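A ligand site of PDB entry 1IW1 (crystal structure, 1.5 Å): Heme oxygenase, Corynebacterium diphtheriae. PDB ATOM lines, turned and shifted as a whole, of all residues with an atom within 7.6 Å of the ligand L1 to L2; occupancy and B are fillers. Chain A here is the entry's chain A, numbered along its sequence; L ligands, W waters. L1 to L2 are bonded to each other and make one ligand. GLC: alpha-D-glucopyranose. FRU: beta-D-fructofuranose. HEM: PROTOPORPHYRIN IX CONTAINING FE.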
ATOM      1  N   LEU A  12     -14.974  28.245  35.226  1.00  0.00           N
ATOM      2  CA  LEU A  12     -15.310  29.087  34.066  1.00  0.00           C
ATOM      3  C   LEU A  12     -16.580  28.681  33.415  1.00  0.00           C
ATOM      4  O   LEU A  12     -17.446  29.512  33.131  1.00  0.00           O
ATOM      5  CB  LEU A  12     -14.227  28.988  32.981  1.00  0.00           C
ATOM      6  CG  LEU A  12     -13.232  30.101  32.940  1.00  0.00           C
ATOM      7  CD1 LEU A  12     -12.149  29.727  31.947  1.00  0.00           C
ATOM      8  CD2 LEU A  12     -13.807  31.506  32.654  1.00  0.00           C
ATOM      9  N   LYS A  13     -16.693  27.380  33.150  1.00  0.00           N
ATOM     10  CA  LYS A  13     -17.881  26.835  32.506  1.00  0.00           C
ATOM     11  C   LYS A  13     -19.137  27.157  33.330  1.00  0.00           C
ATOM     12  O   LYS A  13     -20.143  27.636  32.798  1.00  0.00           O
ATOM     13  CB  LYS A  13     -17.699  25.343  32.296  1.00  0.00           C
ATOM     14  CG  LYS A  13     -18.745  24.700  31.426  1.00  0.00           C
ATOM     15  CD  LYS A  13     -18.366  23.254  31.203  1.00  0.00           C
ATOM     16  CE  LYS A  13     -19.169  22.625  30.129  1.00  0.00           C
ATOM     17  NZ  LYS A  13     -20.465  22.401  30.691  1.00  0.00           N
ATOM     18  N   GLN A  14     -19.057  26.909  34.627  1.00  0.00           N
ATOM     19  CA  GLN A  14     -20.204  27.147  35.479  1.00  0.00           C
ATOM     20  C   GLN A  14     -20.507  28.650  35.670  1.00  0.00           C
ATOM     21  O   GLN A  14     -21.667  29.072  35.621  1.00  0.00           O
ATOM     22  CB  GLN A  14     -20.005  26.479  36.845  1.00  0.00           C
ATOM     23  CG  GLN A  14     -19.868  24.991  36.794  1.00  0.00           C
ATOM     24  CD  GLN A  14     -19.649  24.368  38.175  1.00  0.00           C
ATOM     25  OE1 GLN A  14     -19.026  24.984  39.043  1.00  0.00           O
ATOM     26  NE2 GLN A  14     -20.126  23.145  38.342  1.00  0.00           N
ATOM     27  N   THR A  16     -19.925  31.120  33.721  1.00  0.00           N
ATOM     28  CA  THR A  16     -20.436  31.752  32.512  1.00  0.00           C
ATOM     29  C   THR A  16     -21.640  31.053  31.888  1.00  0.00           C
ATOM     30  O   THR A  16     -22.104  31.441  30.825  1.00  0.00           O
ATOM     31  CB  THR A  16     -19.340  31.848  31.434  1.00  0.00           C
ATOM     32  OG1 THR A  16     -18.893  30.559  31.104  1.00  0.00           O
ATOM     33  CG2 THR A  16     -18.128  32.601  31.873  1.00  0.00           C
ATOM     34  N   ALA A  17     -22.175  30.032  32.544  1.00  0.00           N
ATOM     35  CA  ALA A  17     -23.234  29.248  31.927  1.00  0.00           C
ATOM     36  C   ALA A  17     -24.461  30.105  31.567  1.00  0.00           C
ATOM     37  O   ALA A  17     -25.054  29.944  30.500  1.00  0.00           O
ATOM     38  CB  ALA A  17     -23.626  28.097  32.815  1.00  0.00           C
ATOM     39  N   GLN A  18     -24.881  30.981  32.469  1.00  0.00           N
ATOM     40  CA  GLN A  18     -26.038  31.816  32.196  1.00  0.00           C
ATOM     41  C   GLN A  18     -25.777  32.778  31.047  1.00  0.00           C
ATOM     42  O   GLN A  18     -26.641  33.004  30.190  1.00  0.00           O
ATOM     43  CB  GLN A  18     -26.411  32.606  33.459  1.00  0.00           C
ATOM     44  CG  GLN A  18     -27.615  33.497  33.324  1.00  0.00           C
ATOM     45  CD  GLN A  18     -28.053  34.104  34.630  1.00  0.00           C
ATOM     46  OE1 GLN A  18     -27.289  34.819  35.288  1.00  0.00           O
ATOM     47  NE2 GLN A  18     -29.288  33.839  35.016  1.00  0.00           N
ATOM     48  N   ALA A  19     -24.587  33.370  31.044  1.00  0.00           N
ATOM     49  CA  ALA A  19     -24.227  34.293  29.979  1.00  0.00           C
ATOM     50  C   ALA A  19     -24.096  33.597  28.625  1.00  0.00           C
ATOM     51  O   ALA A  19     -24.426  34.201  27.596  1.00  0.00           O
ATOM     52  CB  ALA A  19     -22.984  35.025  30.330  1.00  0.00           C
ATOM     53  N   HIS A  20     -23.615  32.357  28.634  1.00  0.00           N
ATOM     54  CA  HIS A  20     -23.546  31.552  27.410  1.00  0.00           C
ATOM     55  C   HIS A  20     -24.935  31.275  26.855  1.00  0.00           C
ATOM     56  O   HIS A  20     -25.192  31.476  25.659  1.00  0.00           O
ATOM     57  CB  HIS A  20     -22.783  30.243  27.673  1.00  0.00           C
ATOM     58  CG  HIS A  20     -22.788  29.302  26.514  1.00  0.00           C
ATOM     59  ND1 HIS A  20     -23.793  28.385  26.311  1.00  0.00           N
ATOM     60  CD2 HIS A  20     -21.931  29.155  25.475  1.00  0.00           C
ATOM     61  CE1 HIS A  20     -23.546  27.687  25.222  1.00  0.00           C
ATOM     62  NE2 HIS A  20     -22.450  28.171  24.654  1.00  0.00           N
ATOM     63  N   GLU A  21     -25.863  30.900  27.729  1.00  0.00           N
ATOM     64  CA  GLU A  21     -27.221  30.654  27.302  1.00  0.00           C
ATOM     65  C   GLU A  21     -27.819  31.889  26.664  1.00  0.00           C
ATOM     66  O   GLU A  21     -28.451  31.821  25.622  1.00  0.00           O
ATOM     67  CB  GLU A  21     -28.052  30.199  28.494  1.00  0.00           C
ATOM     68  CG  GLU A  21     -29.508  29.889  28.178  1.00  0.00           C
ATOM     69  CD  GLU A  21     -30.360  31.121  27.901  1.00  0.00           C
ATOM     70  OE1 GLU A  21     -30.266  32.132  28.633  1.00  0.00           O
ATOM     71  OE2 GLU A  21     -31.158  31.102  26.932  1.00  0.00           O
ATOM     72  N   LYS A  22     -27.586  33.057  27.248  1.00  0.00           N
ATOM     73  CA  LYS A  22     -28.116  34.302  26.705  1.00  0.00           C
ATOM     74  C   LYS A  22     -27.574  34.620  25.312  1.00  0.00           C
ATOM     75  O   LYS A  22     -28.298  35.083  24.448  1.00  0.00           O
ATOM     76  CB  LYS A  22     -27.811  35.463  27.652  1.00  0.00           C
ATOM     77  CG  LYS A  22     -28.401  36.782  27.217  1.00  0.00           C
ATOM     78  CD  LYS A  22     -28.215  37.872  28.243  1.00  0.00           C
ATOM     79  CE  LYS A  22     -28.771  39.209  27.791  1.00  0.00           C
ATOM     80  NZ  LYS A  22     -28.448  40.265  28.782  1.00  0.00           N
ATOM     81  N   GLU A  24     -26.088  32.374  23.126  1.00  0.00           N
ATOM     82  CA  GLU A  24     -26.496  31.281  22.235  1.00  0.00           C
ATOM     83  C   GLU A  24     -27.901  31.423  21.732  1.00  0.00           C
ATOM     84  O   GLU A  24     -28.182  31.104  20.578  1.00  0.00           O
ATOM     85  CB  GLU A  24     -26.327  29.938  22.992  1.00  0.00           C
ATOM     86  CG  GLU A  24     -27.149  28.738  22.576  1.00  0.00           C
ATOM     87  CD  GLU A  24     -26.788  27.530  23.423  1.00  0.00           C
ATOM     88  OE1 GLU A  24     -26.679  27.656  24.696  1.00  0.00           O
ATOM     89  OE2 GLU A  24     -26.593  26.464  22.853  1.00  0.00           O
ATOM     90  N   HIS A  25     -28.801  31.896  22.581  1.00  0.00           N
ATOM     91  CA  HIS A  25     -30.222  32.000  22.245  1.00  0.00           C
ATOM     92  C   HIS A  25     -30.680  33.372  21.836  1.00  0.00           C
ATOM     93  O   HIS A  25     -31.893  33.651  21.813  1.00  0.00           O
ATOM     94  CB  HIS A  25     -31.080  31.507  23.420  1.00  0.00           C
ATOM     95  CG  HIS A  25     -30.935  30.056  23.679  1.00  0.00           C
ATOM     96  ND1 HIS A  25     -31.148  29.101  22.704  1.00  0.00           N
ATOM     97  CD2 HIS A  25     -30.525  29.381  24.773  1.00  0.00           C
ATOM     98  CE1 HIS A  25     -30.902  27.907  23.206  1.00  0.00           C
ATOM     99  NE2 HIS A  25     -30.510  28.048  24.460  1.00  0.00           N
ATOM    100  N   TYR A 130     -10.743  32.072  25.733  1.00  0.00           N
ATOM    101  CA  TYR A 130     -11.593  30.935  26.060  1.00  0.00           C
ATOM    102  C   TYR A 130     -12.984  31.117  25.465  1.00  0.00           C
ATOM    103  O   TYR A 130     -13.508  30.226  24.757  1.00  0.00           O
ATOM    104  CB  TYR A 130     -11.699  30.817  27.589  1.00  0.00           C
ATOM    105  CG  TYR A 130     -12.897  30.029  28.096  1.00  0.00           C
ATOM    106  CD1 TYR A 130     -12.912  28.651  28.081  1.00  0.00           C
ATOM    107  CD2 TYR A 130     -14.011  30.703  28.595  1.00  0.00           C
ATOM    108  CE1 TYR A 130     -13.999  27.933  28.563  1.00  0.00           C
ATOM    109  CE2 TYR A 130     -15.105  30.016  29.062  1.00  0.00           C
ATOM    110  CZ  TYR A 130     -15.099  28.622  29.024  1.00  0.00           C
ATOM    111  OH  TYR A 130     -16.206  27.901  29.483  1.00  0.00           O
ATOM    112  N   SER A 138     -16.777  24.566  19.391  1.00  0.00           N
ATOM    113  CA  SER A 138     -17.960  23.905  19.965  1.00  0.00           C
ATOM    114  C   SER A 138     -19.198  24.290  19.150  1.00  0.00           C
ATOM    115  O   SER A 138     -19.457  23.668  18.111  1.00  0.00           O
ATOM    116  CB  SER A 138     -18.067  24.279  21.463  1.00  0.00           C
ATOM    117  OG  SER A 138     -16.918  23.852  22.163  1.00  0.00           O
ATOM    118  N   PHE A 201     -18.956  37.264  27.132  1.00  0.00           N
ATOM    119  CA  PHE A 201     -20.211  36.754  26.634  1.00  0.00           C
ATOM    120  C   PHE A 201     -21.224  37.879  26.461  1.00  0.00           C
ATOM    121  O   PHE A 201     -22.023  37.879  25.538  1.00  0.00           O
ATOM    122  CB  PHE A 201     -20.806  35.720  27.596  1.00  0.00           C
ATOM    123  CG  PHE A 201     -20.322  34.320  27.347  1.00  0.00           C
ATOM    124  CD1 PHE A 201     -19.457  33.686  28.177  1.00  0.00           C
ATOM    125  CD2 PHE A 201     -20.719  33.637  26.210  1.00  0.00           C
ATOM    126  CE1 PHE A 201     -19.026  32.384  27.929  1.00  0.00           C
ATOM    127  CE2 PHE A 201     -20.338  32.348  25.976  1.00  0.00           C
ATOM    128  CZ  PHE A 201     -19.473  31.724  26.792  1.00  0.00           C
HETATM  129  C1  GLC L   1     -26.881  23.947  29.000  1.00  0.00           C
HETATM  130  C2  GLC L   1     -27.813  23.233  29.982  1.00  0.00           C
HETATM  131  C3  GLC L   1     -27.229  21.896  30.392  1.00  0.00           C
HETATM  132  C4  GLC L   1     -27.031  21.053  29.144  1.00  0.00           C
HETATM  133  C5  GLC L   1     -26.129  21.830  28.167  1.00  0.00           C
HETATM  134  C6  GLC L   1     -26.033  21.099  26.827  1.00  0.00           C
HETATM  135  O2  GLC L   1     -28.003  24.111  31.074  1.00  0.00           O
HETATM  136  O3  GLC L   1     -28.097  21.198  31.315  1.00  0.00           O
HETATM  137  O4  GLC L   1     -26.435  19.830  29.496  1.00  0.00           O
HETATM  138  O5  GLC L   1     -26.664  23.111  27.858  1.00  0.00           O
HETATM  139  O6  GLC L   1     -25.170  21.753  25.889  1.00  0.00           O
HETATM  140  C1  FRU L   2     -25.787  26.685  29.414  1.00  0.00           C
HETATM  141  C2  FRU L   2     -24.955  25.429  29.267  1.00  0.00           C
HETATM  142  C3  FRU L   2     -23.646  25.449  30.057  1.00  0.00           C
HETATM  143  C4  FRU L   2     -22.692  24.685  29.168  1.00  0.00           C
HETATM  144  C5  FRU L   2     -23.142  25.219  27.828  1.00  0.00           C
HETATM  145  C6  FRU L   2     -22.739  24.354  26.640  1.00  0.00           C
HETATM  146  O1  FRU L   2     -25.031  27.784  28.894  1.00  0.00           O
HETATM  147  O2  FRU L   2     -25.672  24.252  29.690  1.00  0.00           O
HETATM  148  O3  FRU L   2     -23.782  24.884  31.380  1.00  0.00           O
HETATM  149  O4  FRU L   2     -21.302  24.867  29.438  1.00  0.00           O
HETATM  150  O5  FRU L   2     -24.575  25.311  27.887  1.00  0.00           O
HETATM  151  O6  FRU L   2     -23.006  22.958  26.874  1.00  0.00           O
HETATM  152  CHA HEM L   3     -19.622  25.117  24.339  1.00  0.00           C
HETATM  153  CHB HEM L   3     -18.968  29.867  23.635  1.00  0.00           C
HETATM  154  CHC HEM L   3     -22.734  30.009  20.765  1.00  0.00           C
HETATM  155  CHD HEM L   3     -23.590  25.332  21.584  1.00  0.00           C
HETATM  156  C1A HEM L   3     -19.061  26.447  24.443  1.00  0.00           C
HETATM  157  C2A HEM L   3     -17.908  26.699  25.230  1.00  0.00           C
HETATM  158  C3A HEM L   3     -17.726  28.073  25.023  1.00  0.00           C
HETATM  159  C4A HEM L   3     -18.735  28.608  24.164  1.00  0.00           C
HETATM  160  CMA HEM L   3     -16.692  29.009  25.620  1.00  0.00           C
HETATM  161  CAA HEM L   3     -17.063  25.828  26.082  1.00  0.00           C
HETATM  162  CBA HEM L   3     -17.660  25.491  27.395  1.00  0.00           C
HETATM  163  CGA HEM L   3     -16.678  24.745  28.243  1.00  0.00           C
HETATM  164  O1A HEM L   3     -16.490  23.498  28.030  1.00  0.00           O
HETATM  165  O2A HEM L   3     -16.048  25.321  29.182  1.00  0.00           O
HETATM  166  C1B HEM L   3     -19.852  30.412  22.830  1.00  0.00           C
HETATM  167  C2B HEM L   3     -20.045  31.727  22.322  1.00  0.00           C
HETATM  168  C3B HEM L   3     -21.047  31.812  21.542  1.00  0.00           C
HETATM  169  C4B HEM L   3     -21.636  30.416  21.539  1.00  0.00           C
HETATM  170  CMB HEM L   3     -19.091  32.805  22.695  1.00  0.00           C
HETATM  171  CAB HEM L   3     -21.654  32.923  20.792  1.00  0.00           C
HETATM  172  CBB HEM L   3     -20.866  34.056  20.368  1.00  0.00           C
HETATM  173  C1C HEM L   3     -23.291  28.748  20.697  1.00  0.00           C
HETATM  174  C2C HEM L   3     -24.333  28.400  19.802  1.00  0.00           C
HETATM  175  C3C HEM L   3     -24.640  27.117  20.108  1.00  0.00           C
HETATM  176  C4C HEM L   3     -23.731  26.571  21.055  1.00  0.00           C
HETATM  177  CMC HEM L   3     -25.136  29.317  18.910  1.00  0.00           C
HETATM  178  CAC HEM L   3     -25.761  26.266  19.463  1.00  0.00           C
HETATM  179  CBC HEM L   3     -25.335  25.766  18.286  1.00  0.00           C
HETATM  180  C1D HEM L   3     -22.623  24.829  22.374  1.00  0.00           C
HETATM  181  C2D HEM L   3     -22.387  23.521  22.859  1.00  0.00           C
HETATM  182  C3D HEM L   3     -21.264  23.408  23.655  1.00  0.00           C
HETATM  183  C4D HEM L   3     -20.745  24.786  23.619  1.00  0.00           C
HETATM  184  CMD HEM L   3     -23.368  22.390  22.507  1.00  0.00           C
HETATM  185  CAD HEM L   3     -20.746  22.239  24.328  1.00  0.00           C
HETATM  186  CBD HEM L   3     -19.545  21.607  23.630  1.00  0.00           C
HETATM  187  CGD HEM L   3     -19.823  21.033  22.322  1.00  0.00           C
HETATM  188  O1D HEM L   3     -20.872  20.336  22.189  1.00  0.00           O
HETATM  189  O2D HEM L   3     -19.109  21.135  21.284  1.00  0.00           O
HETATM  190  NA  HEM L   3     -19.569  27.520  23.778  1.00  0.00           N
HETATM  191  NB  HEM L   3     -20.885  29.630  22.289  1.00  0.00           N
HETATM  192  NC  HEM L   3     -22.877  27.688  21.419  1.00  0.00           N
HETATM  193  ND  HEM L   3     -21.568  25.594  22.891  1.00  0.00           N
HETATM  194 FE   HEM L   3     -21.390  27.640  22.806  1.00  0.00          FE
HETATM  195  O   HOH W   1     -20.829  27.473  30.094  1.00  0.00           O
HETATM  196  O   HOH W   2     -26.563  25.411  25.847  1.00  0.00           O
HETATM  197  O   HOH W   3     -21.765  20.917  28.072  1.00  0.00           O
HETATM  198  O   HOH W   4     -23.733  20.076  29.942  1.00  0.00           O
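O of Ala 17 sits at hydrogen-bond distance from O1 of FRU L2, 2.7 Å away.
The side-chain amino group (NZ) of Lys 13 sits at hydrogen-bond distance from an oxygen (O4) of FRU L2 (2.9 Å).
An oxygen (O1) of FRU L2 is in hydrogen-bond range of a ring nitrogen (ND1) of His 20, 2.9 Å away.
The backbone NH of Glu 21 sits at hydrogen-bond distance from an oxygen (O1) of FRU L2 (3.4 Å).
A ring nitrogen (NE2) of His 20 binds an iron atom (FE) of HEM L3 (2.2 Å).
O2A of HEM L3 sits at hydrogen-bond distance from OH of Tyr 130, at 2.6 Å.
Water W3 bridges O6 of FRU L2 (2.7 Å) and NZ of Lys 13 (3.3 Å).
Water W1 bridges O4 of FRU L2 and O of Lys 13.
Water W2 lies within hydrogen-bond range of the side-chain carboxylate (OE1) of Glu 24 and an oxygen (O5) of FRU L2.
Hydrophobic or aromatic side chains that line the ligand L1 to L2: Ala 17 and His 20.
Within 4 Å of the ligand L1 to L2: Lys 13, Ala 17, His 20 and Glu 21.
The nearest printed residue that does not touch the ligand L1 to L2 is Glu 24 (4.5 Å).
A ring nitrogen (ND1) of His 20 lies close to the side-chain carboxylate of Glu 24, 3.4 Å away.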
